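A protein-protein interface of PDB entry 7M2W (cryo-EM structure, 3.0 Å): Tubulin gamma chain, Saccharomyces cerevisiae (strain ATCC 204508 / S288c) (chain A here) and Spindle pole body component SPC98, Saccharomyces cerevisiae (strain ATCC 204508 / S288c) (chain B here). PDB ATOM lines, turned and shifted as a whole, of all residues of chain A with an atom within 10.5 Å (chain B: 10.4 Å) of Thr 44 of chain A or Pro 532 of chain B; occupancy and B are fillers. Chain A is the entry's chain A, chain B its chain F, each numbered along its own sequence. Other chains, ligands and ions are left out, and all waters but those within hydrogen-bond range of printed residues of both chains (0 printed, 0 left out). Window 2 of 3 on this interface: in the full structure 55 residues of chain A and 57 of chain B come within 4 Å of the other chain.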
ATOM      1  N   SER A  37     -13.948 -19.386  26.069  1.00  0.00           N
ATOM      2  CA  SER A  37     -12.713 -19.268  25.304  1.00  0.00           C
ATOM      3  C   SER A  37     -11.490 -19.345  26.206  1.00  0.00           C
ATOM      4  O   SER A  37     -11.432 -18.699  27.255  1.00  0.00           O
ATOM      5  CB  SER A  37     -12.711 -17.954  24.523  1.00  0.00           C
ATOM      6  OG  SER A  37     -13.073 -16.869  25.358  1.00  0.00           O
ATOM      7  N   GLN A  38     -10.512 -20.144  25.788  1.00  0.00           N
ATOM      8  CA  GLN A  38      -9.271 -20.323  26.527  1.00  0.00           C
ATOM      9  C   GLN A  38      -8.322 -19.144  26.381  1.00  0.00           C
ATOM     10  O   GLN A  38      -7.164 -19.246  26.795  1.00  0.00           O
ATOM     11  CB  GLN A  38      -8.566 -21.605  26.073  1.00  0.00           C
ATOM     12  CG  GLN A  38      -9.466 -22.824  26.015  1.00  0.00           C
ATOM     13  CD  GLN A  38     -10.028 -23.195  27.369  1.00  0.00           C
ATOM     14  OE1 GLN A  38      -9.294 -23.298  28.352  1.00  0.00           O
ATOM     15  NE2 GLN A  38     -11.339 -23.401  27.430  1.00  0.00           N
ATOM     16  N   LEU A  39      -8.773 -18.046  25.806  1.00  0.00           N
ATOM     17  CA  LEU A  39      -7.843 -16.943  25.645  1.00  0.00           C
ATOM     18  C   LEU A  39      -7.915 -15.997  26.835  1.00  0.00           C
ATOM     19  O   LEU A  39      -8.968 -15.854  27.463  1.00  0.00           O
ATOM     20  CB  LEU A  39      -8.153 -16.168  24.369  1.00  0.00           C
ATOM     21  CG  LEU A  39      -7.795 -16.838  23.046  1.00  0.00           C
ATOM     22  CD1 LEU A  39      -7.862 -15.822  21.926  1.00  0.00           C
ATOM     23  CD2 LEU A  39      -6.419 -17.475  23.122  1.00  0.00           C
ATOM     24  N   PRO A  40      -6.805 -15.344  27.162  1.00  0.00           N
ATOM     25  CA  PRO A  40      -6.844 -14.301  28.186  1.00  0.00           C
ATOM     26  C   PRO A  40      -7.342 -12.991  27.605  1.00  0.00           C
ATOM     27  O   PRO A  40      -7.132 -12.685  26.428  1.00  0.00           O
ATOM     28  CB  PRO A  40      -5.383 -14.195  28.633  1.00  0.00           C
ATOM     29  CG  PRO A  40      -4.615 -14.551  27.403  1.00  0.00           C
ATOM     30  CD  PRO A  40      -5.438 -15.581  26.665  1.00  0.00           C
ATOM     31  N   ASP A  41      -8.009 -12.208  28.447  1.00  0.00           N
ATOM     32  CA  ASP A  41      -8.527 -10.911  28.034  1.00  0.00           C
ATOM     33  C   ASP A  41      -7.439  -9.852  27.898  1.00  0.00           C
ATOM     34  O   ASP A  41      -7.760  -8.676  27.706  1.00  0.00           O
ATOM     35  CB  ASP A  41      -9.607 -10.437  29.016  1.00  0.00           C
ATOM     36  CG  ASP A  41      -9.106 -10.353  30.445  1.00  0.00           C
ATOM     37  OD1 ASP A  41      -7.945 -10.738  30.700  1.00  0.00           O
ATOM     38  OD2 ASP A  41      -9.877  -9.902  31.319  1.00  0.00           O
ATOM     39  N   SER A  42      -6.164 -10.243  27.989  1.00  0.00           N
ATOM     40  CA  SER A  42      -5.072  -9.320  27.712  1.00  0.00           C
ATOM     41  C   SER A  42      -4.873  -9.101  26.219  1.00  0.00           C
ATOM     42  O   SER A  42      -4.531  -7.988  25.808  1.00  0.00           O
ATOM     43  CB  SER A  42      -3.776  -9.837  28.339  1.00  0.00           C
ATOM     44  OG  SER A  42      -3.465 -11.138  27.872  1.00  0.00           O
ATOM     45  N   SER A  43      -5.077 -10.135  25.404  1.00  0.00           N
ATOM     46  CA  SER A  43      -4.975 -10.042  23.949  1.00  0.00           C
ATOM     47  C   SER A  43      -6.340 -10.390  23.363  1.00  0.00           C
ATOM     48  O   SER A  43      -6.644 -11.565  23.135  1.00  0.00           O
ATOM     49  CB  SER A  43      -3.887 -10.965  23.412  1.00  0.00           C
ATOM     50  OG  SER A  43      -3.501 -10.594  22.100  1.00  0.00           O
ATOM     51  N   THR A  44      -7.161  -9.370  23.127  1.00  0.00           N
ATOM     52  CA  THR A  44      -8.482  -9.538  22.538  1.00  0.00           C
ATOM     53  C   THR A  44      -8.442  -9.684  21.025  1.00  0.00           C
ATOM     54  O   THR A  44      -9.497  -9.839  20.401  1.00  0.00           O
ATOM     55  CB  THR A  44      -9.379  -8.351  22.906  1.00  0.00           C
ATOM     56  OG1 THR A  44     -10.714  -8.595  22.446  1.00  0.00           O
ATOM     57  CG2 THR A  44      -8.854  -7.078  22.268  1.00  0.00           C
ATOM     58  N   GLU A  45      -7.259  -9.638  20.420  1.00  0.00           N
ATOM     59  CA  GLU A  45      -7.150  -9.626  18.971  1.00  0.00           C
ATOM     60  C   GLU A  45      -7.299 -11.031  18.406  1.00  0.00           C
ATOM     61  O   GLU A  45      -6.509 -11.930  18.710  1.00  0.00           O
ATOM     62  CB  GLU A  45      -5.810  -9.027  18.546  1.00  0.00           C
ATOM     63  CG  GLU A  45      -5.433  -7.725  19.261  1.00  0.00           C
ATOM     64  CD  GLU A  45      -6.520  -6.653  19.235  1.00  0.00           C
ATOM     65  OE1 GLU A  45      -6.426  -5.709  20.047  1.00  0.00           O
ATOM     66  OE2 GLU A  45      -7.435  -6.713  18.386  1.00  0.00           O
ATOM     67  N   ARG A  46      -8.324 -11.213  17.578  1.00  0.00           N
ATOM     68  CA  ARG A  46      -8.577 -12.477  16.905  1.00  0.00           C
ATOM     69  C   ARG A  46      -8.479 -12.265  15.403  1.00  0.00           C
ATOM     70  O   ARG A  46      -8.942 -11.247  14.884  1.00  0.00           O
ATOM     71  CB  ARG A  46      -9.964 -13.033  17.256  1.00  0.00           C
ATOM     72  CG  ARG A  46     -10.232 -13.185  18.740  1.00  0.00           C
ATOM     73  CD  ARG A  46      -9.866 -14.574  19.214  1.00  0.00           C
ATOM     74  NE  ARG A  46     -10.871 -15.561  18.835  1.00  0.00           N
ATOM     75  CZ  ARG A  46     -11.563 -16.291  19.702  1.00  0.00           C
ATOM     76  NH1 ARG A  46     -11.357 -16.150  21.004  1.00  0.00           N
ATOM     77  NH2 ARG A  46     -12.457 -17.165  19.268  1.00  0.00           N
ATOM     78  N   ASP A  47      -7.867 -13.224  14.709  1.00  0.00           N
ATOM     79  CA  ASP A  47      -7.925 -13.255  13.254  1.00  0.00           C
ATOM     80  C   ASP A  47      -8.648 -14.495  12.745  1.00  0.00           C
ATOM     81  O   ASP A  47      -8.769 -14.674  11.527  1.00  0.00           O
ATOM     82  CB  ASP A  47      -6.521 -13.154  12.635  1.00  0.00           C
ATOM     83  CG  ASP A  47      -5.600 -14.291  13.047  1.00  0.00           C
ATOM     84  OD1 ASP A  47      -4.467 -13.994  13.482  1.00  0.00           O
ATOM     85  OD2 ASP A  47      -5.980 -15.473  12.916  1.00  0.00           O
ATOM     86  N   ASP A  48      -9.129 -15.348  13.640  1.00  0.00           N
ATOM     87  CA  ASP A  48      -9.964 -16.480  13.282  1.00  0.00           C
ATOM     88  C   ASP A  48     -11.393 -16.020  13.036  1.00  0.00           C
ATOM     89  O   ASP A  48     -11.743 -14.858  13.253  1.00  0.00           O
ATOM     90  CB  ASP A  48      -9.927 -17.551  14.378  1.00  0.00           C
ATOM     91  CG  ASP A  48     -10.332 -17.016  15.741  1.00  0.00           C
ATOM     92  OD1 ASP A  48     -10.850 -15.884  15.826  1.00  0.00           O
ATOM     93  OD2 ASP A  48     -10.129 -17.734  16.739  1.00  0.00           O
ATOM     94  N   GLU A  56     -22.323 -17.049  19.521  1.00  0.00           N
ATOM     95  CA  GLU A  56     -21.798 -16.308  20.657  1.00  0.00           C
ATOM     96  C   GLU A  56     -22.876 -15.396  21.225  1.00  0.00           C
ATOM     97  O   GLU A  56     -23.368 -14.500  20.532  1.00  0.00           O
ATOM     98  CB  GLU A  56     -20.571 -15.496  20.236  1.00  0.00           C
ATOM     99  CG  GLU A  56     -19.813 -14.853  21.375  1.00  0.00           C
ATOM    100  CD  GLU A  56     -18.840 -13.797  20.897  1.00  0.00           C
ATOM    101  OE1 GLU A  56     -18.794 -13.542  19.675  1.00  0.00           O
ATOM    102  OE2 GLU A  56     -18.117 -13.225  21.739  1.00  0.00           O
ATOM    103  N   ARG A  59     -19.971 -12.936  25.869  1.00  0.00           N
ATOM    104  CA  ARG A  59     -18.837 -12.399  25.128  1.00  0.00           C
ATOM    105  C   ARG A  59     -17.660 -13.364  25.076  1.00  0.00           C
ATOM    106  O   ARG A  59     -16.686 -13.094  24.365  1.00  0.00           O
ATOM    107  CB  ARG A  59     -18.405 -11.062  25.731  1.00  0.00           C
ATOM    108  CG  ARG A  59     -19.499  -9.989  25.760  1.00  0.00           C
ATOM    109  CD  ARG A  59     -19.798  -9.365  24.384  1.00  0.00           C
ATOM    110  NE  ARG A  59     -20.272 -10.303  23.363  1.00  0.00           N
ATOM    111  CZ  ARG A  59     -21.397 -11.013  23.440  1.00  0.00           C
ATOM    112  NH1 ARG A  59     -22.201 -10.898  24.489  1.00  0.00           N
ATOM    113  NH2 ARG A  59     -21.727 -11.837  22.455  1.00  0.00           N
ATOM    114  N   ASN A  60     -17.720 -14.480  25.806  1.00  0.00           N
ATOM    115  CA  ASN A  60     -16.687 -15.505  25.735  1.00  0.00           C
ATOM    116  C   ASN A  60     -17.258 -16.919  25.747  1.00  0.00           C
ATOM    117  O   ASN A  60     -16.514 -17.875  25.979  1.00  0.00           O
ATOM    118  CB  ASN A  60     -15.682 -15.337  26.875  1.00  0.00           C
ATOM    119  CG  ASN A  60     -15.115 -13.936  26.950  1.00  0.00           C
ATOM    120  OD1 ASN A  60     -15.126 -13.306  28.007  1.00  0.00           O
ATOM    121  ND2 ASN A  60     -14.614 -13.441  25.825  1.00  0.00           N
ATOM    122  N   PHE A  62     -19.177 -19.802  23.450  1.00  0.00           N
ATOM    123  CA  PHE A  62     -19.552 -20.217  22.110  1.00  0.00           C
ATOM    124  C   PHE A  62     -20.324 -21.524  22.181  1.00  0.00           C
ATOM    125  O   PHE A  62     -19.955 -22.435  22.930  1.00  0.00           O
ATOM    126  CB  PHE A  62     -18.322 -20.383  21.212  1.00  0.00           C
ATOM    127  CG  PHE A  62     -17.485 -19.142  21.096  1.00  0.00           C
ATOM    128  CD1 PHE A  62     -16.486 -18.875  22.015  1.00  0.00           C
ATOM    129  CD2 PHE A  62     -17.702 -18.241  20.071  1.00  0.00           C
ATOM    130  CE1 PHE A  62     -15.718 -17.735  21.909  1.00  0.00           C
ATOM    131  CE2 PHE A  62     -16.939 -17.100  19.961  1.00  0.00           C
ATOM    132  CZ  PHE A  62     -15.945 -16.847  20.882  1.00  0.00           C
ATOM    133  N   TYR A 362      -3.621 -20.651  17.817  1.00  0.00           N
ATOM    134  CA  TYR A 362      -3.774 -21.089  19.195  1.00  0.00           C
ATOM    135  C   TYR A 362      -3.321 -22.525  19.400  1.00  0.00           C
ATOM    136  O   TYR A 362      -3.151 -22.952  20.547  1.00  0.00           O
ATOM    137  CB  TYR A 362      -5.228 -20.921  19.633  1.00  0.00           C
ATOM    138  CG  TYR A 362      -5.833 -19.630  19.146  1.00  0.00           C
ATOM    139  CD1 TYR A 362      -6.702 -19.614  18.067  1.00  0.00           C
ATOM    140  CD2 TYR A 362      -5.517 -18.421  19.749  1.00  0.00           C
ATOM    141  CE1 TYR A 362      -7.249 -18.437  17.610  1.00  0.00           C
ATOM    142  CE2 TYR A 362      -6.059 -17.237  19.297  1.00  0.00           C
ATOM    143  CZ  TYR A 362      -6.925 -17.252  18.229  1.00  0.00           C
ATOM    144  OH  TYR A 362      -7.470 -16.077  17.771  1.00  0.00           O
ATOM    145  N   LYS B 467       1.526   2.945  19.507  1.00  0.00           N
ATOM    146  CA  LYS B 467       0.617   4.054  19.775  1.00  0.00           C
ATOM    147  C   LYS B 467      -0.252   4.431  18.590  1.00  0.00           C
ATOM    148  O   LYS B 467      -1.408   4.814  18.781  1.00  0.00           O
ATOM    149  CB  LYS B 467       1.406   5.286  20.235  1.00  0.00           C
ATOM    150  CG  LYS B 467       0.536   6.414  20.754  1.00  0.00           C
ATOM    151  CD  LYS B 467       1.373   7.592  21.216  1.00  0.00           C
ATOM    152  CE  LYS B 467       0.535   8.856  21.312  1.00  0.00           C
ATOM    153  NZ  LYS B 467       1.352  10.039  21.699  1.00  0.00           N
ATOM    154  N   HIS B 469      -0.427   2.189  15.885  1.00  0.00           N
ATOM    155  CA  HIS B 469      -0.732   0.903  15.259  1.00  0.00           C
ATOM    156  C   HIS B 469      -0.221   0.844  13.823  1.00  0.00           C
ATOM    157  O   HIS B 469      -0.991   0.721  12.872  1.00  0.00           O
ATOM    158  CB  HIS B 469      -2.231   0.616  15.316  1.00  0.00           C
ATOM    159  CG  HIS B 469      -2.894   1.115  16.561  1.00  0.00           C
ATOM    160  ND1 HIS B 469      -2.521   0.701  17.822  1.00  0.00           N
ATOM    161  CD2 HIS B 469      -3.907   1.996  16.739  1.00  0.00           C
ATOM    162  CE1 HIS B 469      -3.275   1.306  18.722  1.00  0.00           C
ATOM    163  NE2 HIS B 469      -4.124   2.097  18.091  1.00  0.00           N
ATOM    164  N   ASP B 472      -0.458  -2.884  12.441  1.00  0.00           N
ATOM    165  CA  ASP B 472      -1.874  -3.193  12.291  1.00  0.00           C
ATOM    166  C   ASP B 472      -2.473  -2.487  11.086  1.00  0.00           C
ATOM    167  O   ASP B 472      -3.282  -3.075  10.365  1.00  0.00           O
ATOM    168  CB  ASP B 472      -2.631  -2.811  13.560  1.00  0.00           C
ATOM    169  CG  ASP B 472      -2.283  -3.699  14.734  1.00  0.00           C
ATOM    170  OD1 ASP B 472      -1.944  -4.878  14.506  1.00  0.00           O
ATOM    171  OD2 ASP B 472      -2.348  -3.220  15.884  1.00  0.00           O
ATOM    172  N   SER B 524     -14.087 -11.271   9.645  1.00  0.00           N
ATOM    173  CA  SER B 524     -13.019 -11.418  10.625  1.00  0.00           C
ATOM    174  C   SER B 524     -12.464 -10.084  11.111  1.00  0.00           C
ATOM    175  O   SER B 524     -11.769 -10.061  12.131  1.00  0.00           O
ATOM    176  CB  SER B 524     -11.891 -12.269  10.041  1.00  0.00           C
ATOM    177  OG  SER B 524     -11.290 -11.632   8.928  1.00  0.00           O
ATOM    178  N   LEU B 525     -12.753  -8.982  10.416  1.00  0.00           N
ATOM    179  CA  LEU B 525     -12.323  -7.670  10.881  1.00  0.00           C
ATOM    180  C   LEU B 525     -13.155  -7.173  12.056  1.00  0.00           C
ATOM    181  O   LEU B 525     -12.833  -6.126  12.630  1.00  0.00           O
ATOM    182  CB  LEU B 525     -12.383  -6.661   9.736  1.00  0.00           C
ATOM    183  CG  LEU B 525     -11.695  -7.056   8.428  1.00  0.00           C
ATOM    184  CD1 LEU B 525     -11.630  -5.867   7.489  1.00  0.00           C
ATOM    185  CD2 LEU B 525     -10.302  -7.599   8.692  1.00  0.00           C
ATOM    186  N   ARG B 526     -14.218  -7.891  12.421  1.00  0.00           N
ATOM    187  CA  ARG B 526     -15.034  -7.487  13.558  1.00  0.00           C
ATOM    188  C   ARG B 526     -14.273  -7.583  14.871  1.00  0.00           C
ATOM    189  O   ARG B 526     -14.608  -6.869  15.821  1.00  0.00           O
ATOM    190  CB  ARG B 526     -16.303  -8.335  13.618  1.00  0.00           C
ATOM    191  CG  ARG B 526     -16.080  -9.737  14.147  1.00  0.00           C
ATOM    192  CD  ARG B 526     -17.335 -10.578  14.045  1.00  0.00           C
ATOM    193  NE  ARG B 526     -17.187 -11.838  14.763  1.00  0.00           N
ATOM    194  CZ  ARG B 526     -16.672 -12.944  14.239  1.00  0.00           C
ATOM    195  NH1 ARG B 526     -16.254 -12.953  12.982  1.00  0.00           N
ATOM    196  NH2 ARG B 526     -16.579 -14.043  14.973  1.00  0.00           N
ATOM    197  N   HIS B 527     -13.259  -8.444  14.949  1.00  0.00           N
ATOM    198  CA  HIS B 527     -12.390  -8.462  16.116  1.00  0.00           C
ATOM    199  C   HIS B 527     -11.535  -7.213  16.203  1.00  0.00           C
ATOM    200  O   HIS B 527     -11.038  -6.885  17.285  1.00  0.00           O
ATOM    201  CB  HIS B 527     -11.481  -9.689  16.085  1.00  0.00           C
ATOM    202  CG  HIS B 527     -12.204 -10.967  15.804  1.00  0.00           C
ATOM    203  ND1 HIS B 527     -13.042 -11.565  16.720  1.00  0.00           N
ATOM    204  CD2 HIS B 527     -12.213 -11.761  14.709  1.00  0.00           C
ATOM    205  CE1 HIS B 527     -13.536 -12.674  16.201  1.00  0.00           C
ATOM    206  NE2 HIS B 527     -13.050 -12.815  14.981  1.00  0.00           N
ATOM    207  N   LEU B 528     -11.350  -6.517  15.086  1.00  0.00           N
ATOM    208  CA  LEU B 528     -10.574  -5.289  15.056  1.00  0.00           C
ATOM    209  C   LEU B 528     -11.452  -4.064  15.276  1.00  0.00           C
ATOM    210  O   LEU B 528     -11.057  -3.143  15.996  1.00  0.00           O
ATOM    211  CB  LEU B 528      -9.829  -5.182  13.725  1.00  0.00           C
ATOM    212  CG  LEU B 528      -8.613  -4.265  13.661  1.00  0.00           C
ATOM    213  CD1 LEU B 528      -7.539  -4.753  14.615  1.00  0.00           C
ATOM    214  CD2 LEU B 528      -8.087  -4.212  12.242  1.00  0.00           C
ATOM    215  N   MET B 529     -12.641  -4.041  14.669  1.00  0.00           N
ATOM    216  CA  MET B 529     -13.544  -2.911  14.871  1.00  0.00           C
ATOM    217  C   MET B 529     -14.053  -2.850  16.304  1.00  0.00           C
ATOM    218  O   MET B 529     -14.159  -1.761  16.878  1.00  0.00           O
ATOM    219  CB  MET B 529     -14.725  -2.987  13.906  1.00  0.00           C
ATOM    220  CG  MET B 529     -15.669  -1.800  14.011  1.00  0.00           C
ATOM    221  SD  MET B 529     -16.878  -1.712  12.679  1.00  0.00           S
ATOM    222  CE  MET B 529     -17.763  -3.245  12.936  1.00  0.00           C
ATOM    223  N   ASN B 530     -14.369  -3.998  16.897  1.00  0.00           N
ATOM    224  CA  ASN B 530     -14.863  -4.063  18.263  1.00  0.00           C
ATOM    225  C   ASN B 530     -13.745  -4.231  19.280  1.00  0.00           C
ATOM    226  O   ASN B 530     -13.985  -4.759  20.369  1.00  0.00           O
ATOM    227  CB  ASN B 530     -15.873  -5.204  18.409  1.00  0.00           C
ATOM    228  CG  ASN B 530     -16.894  -5.224  17.291  1.00  0.00           C
ATOM    229  OD1 ASN B 530     -17.553  -4.222  17.018  1.00  0.00           O
ATOM    230  ND2 ASN B 530     -17.043  -6.374  16.646  1.00  0.00           N
ATOM    231  N   SER B 531     -12.536  -3.803  18.949  1.00  0.00           N
ATOM    232  CA  SER B 531     -11.417  -3.920  19.871  1.00  0.00           C
ATOM    233  C   SER B 531     -11.339  -2.673  20.740  1.00  0.00           C
ATOM    234  O   SER B 531     -11.658  -1.578  20.263  1.00  0.00           O
ATOM    235  CB  SER B 531     -10.116  -4.114  19.107  1.00  0.00           C
ATOM    236  OG  SER B 531      -9.032  -4.333  19.990  1.00  0.00           O
ATOM    237  N   PRO B 532     -10.932  -2.785  22.004  1.00  0.00           N
ATOM    238  CA  PRO B 532     -10.870  -1.590  22.860  1.00  0.00           C
ATOM    239  C   PRO B 532      -9.840  -0.570  22.414  1.00  0.00           C
ATOM    240  O   PRO B 532      -9.968   0.613  22.752  1.00  0.00           O
ATOM    241  CB  PRO B 532     -10.529  -2.168  24.241  1.00  0.00           C
ATOM    242  CG  PRO B 532     -10.892  -3.614  24.160  1.00  0.00           C
ATOM    243  CD  PRO B 532     -10.619  -4.011  22.750  1.00  0.00           C
ATOM    244  N   ARG B 533      -8.819  -0.985  21.664  1.00  0.00           N
ATOM    245  CA  ARG B 533      -7.743  -0.083  21.277  1.00  0.00           C
ATOM    246  C   ARG B 533      -7.573   0.084  19.776  1.00  0.00           C
ATOM    247  O   ARG B 533      -7.310   1.199  19.322  1.00  0.00           O
ATOM    248  CB  ARG B 533      -6.414  -0.557  21.879  1.00  0.00           C
ATOM    249  CG  ARG B 533      -6.083  -2.014  21.611  1.00  0.00           C
ATOM    250  CD  ARG B 533      -4.719  -2.364  22.179  1.00  0.00           C
ATOM    251  NE  ARG B 533      -4.317  -3.731  21.859  1.00  0.00           N
ATOM    252  CZ  ARG B 533      -3.599  -4.066  20.793  1.00  0.00           C
ATOM    253  NH1 ARG B 533      -3.201  -3.132  19.941  1.00  0.00           N
ATOM    254  NH2 ARG B 533      -3.276  -5.333  20.580  1.00  0.00           N
ATOM    255  N   ASN B 534      -7.719  -0.984  18.993  1.00  0.00           N
ATOM    256  CA  ASN B 534      -7.414  -0.953  17.569  1.00  0.00           C
ATOM    257  C   ASN B 534      -8.614  -0.606  16.697  1.00  0.00           C
ATOM    258  O   ASN B 534      -8.554  -0.807  15.481  1.00  0.00           O
ATOM    259  CB  ASN B 534      -6.826  -2.292  17.127  1.00  0.00           C
ATOM    260  CG  ASN B 534      -5.630  -2.703  17.954  1.00  0.00           C
ATOM    261  OD1 ASN B 534      -5.027  -1.882  18.643  1.00  0.00           O
ATOM    262  ND2 ASN B 534      -5.276  -3.980  17.887  1.00  0.00           N
ATOM    263  N   SER B 535      -9.704  -0.103  17.278  1.00  0.00           N
ATOM    264  CA  SER B 535     -10.822   0.353  16.459  1.00  0.00           C
ATOM    265  C   SER B 535     -10.415   1.472  15.511  1.00  0.00           C
ATOM    266  O   SER B 535     -10.975   1.581  14.412  1.00  0.00           O
ATOM    267  CB  SER B 535     -11.974   0.822  17.347  1.00  0.00           C
ATOM    268  OG  SER B 535     -12.842   1.688  16.636  1.00  0.00           O
ATOM    269  N   SER B 536      -9.452   2.305  15.913  1.00  0.00           N
ATOM    270  CA  SER B 536      -8.959   3.365  15.043  1.00  0.00           C
ATOM    271  C   SER B 536      -8.370   2.823  13.750  1.00  0.00           C
ATOM    272  O   SER B 536      -8.314   3.554  12.756  1.00  0.00           O
ATOM    273  CB  SER B 536      -7.916   4.199  15.784  1.00  0.00           C
ATOM    274  OG  SER B 536      -7.013   3.365  16.488  1.00  0.00           O
ATOM    275  N   VAL B 537      -7.926   1.567  13.742  1.00  0.00           N
ATOM    276  CA  VAL B 537      -7.402   0.968  12.521  1.00  0.00           C
ATOM    277  C   VAL B 537      -8.492   0.872  11.464  1.00  0.00           C
ATOM    278  O   VAL B 537      -8.260   1.147  10.282  1.00  0.00           O
ATOM    279  CB  VAL B 537      -6.786  -0.409  12.823  1.00  0.00           C
ATOM    280  CG1 VAL B 537      -6.244  -1.033  11.552  1.00  0.00           C
ATOM    281  CG2 VAL B 537      -5.699  -0.284  13.873  1.00  0.00           C
ATOM    282  N   ASN B 539     -11.348   2.608  11.679  1.00  0.00           N
ATOM    283  CA  ASN B 539     -11.893   3.951  11.503  1.00  0.00           C
ATOM    284  C   ASN B 539     -11.457   4.589  10.189  1.00  0.00           C
ATOM    285  O   ASN B 539     -12.166   5.459   9.672  1.00  0.00           O
ATOM    286  CB  ASN B 539     -11.483   4.852  12.670  1.00  0.00           C
ATOM    287  CG  ASN B 539     -12.158   4.466  13.972  1.00  0.00           C
ATOM    288  OD1 ASN B 539     -13.045   3.614  13.998  1.00  0.00           O
ATOM    289  ND2 ASN B 539     -11.750   5.108  15.061  1.00  0.00           N
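The backbone carbonyl oxygen (O) of Asp 48 of chain A sits at hydrogen-bond distance from a ring nitrogen (NE2) of His 527 of chain B (3.0 Å). The side-chain hydroxyl (OG) of Ser 531 of chain B sits at hydrogen-bond distance from the side-chain carboxylate (OE1) of Glu 45 of chain A (2.9 Å). OE1 of Glu 45 of chain A is in salt-bridge range of NH2 of Arg 533 of chain B, at 3.2 Å. The side-chain carboxylate (OE1) of Glu 45 of chain A lies within hydrogen-bond range of the side-chain amide nitrogen (ND2) of Asn 534 of chain B (3.0 Å).
The guanidinium group of Arg 46 of chain A is in salt-bridge range of the side-chain carboxylate of Asp 48 of chain A (3.0 Å). OD1 of Asn 534 of chain B lies within hydrogen-bond range of NH1 of Arg 533 of chain B (2.6 Å). The side-chain carboxylate of Asp 48 of chain A lies close to the side-chain hydroxyl of Tyr 362 of chain A (3.3 Å).
Ser 531 of chain B touches Thr 44 of chain A (OG to CG2, 3.6 Å). Thr 44 of chain A touches Pro 532 of chain B (CG2 to CD, 3.6 Å). His 527 of chain B touches Glu 45 of chain A (O to OE2, 3.8 Å). Arg 46 of chain A touches His 527 of chain B.
Of chain B, only Ser 531 and Pro 532 come within 4 Å of Thr 44 of chain A. Of chain A, only Thr 44 comes within 4 Å of Pro 532 of chain B. Of chain A, only Thr 44 (3.6 Å) and Glu 45 (2.9 Å) come within 4 Å of Ser 531 of chain B. Of the printed residues of chain A, Arg 533 of chain B touches Glu 45. Printed residues of chain B within 4 Å of Asp 48 of chain A: His 527 (3.0 Å). Of the printed residues of chain A, Asn 534 of chain B touches Glu 45. His 469 of chain B touches none of the printed residues of chain A. The nearest residue of chain B that does not touch Thr 44 of chain A is His 527 of chain B (4.6 Å). The nearest residue of chain A that does not touch Pro 532 of chain B is Glu 45 of chain A (5.3 Å).
Of the 17 printed residues of chain A, 4 touch a printed residue of chain B. Printed residues of chain A that touch a printed residue of chain B: Thr 44, Glu 45, Arg 46 and Asp 48. Along chain B the printed residues that touch a printed residue of chain A span positions 527 to 534. Among the printed residues, 8 pairs touch across the chains.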
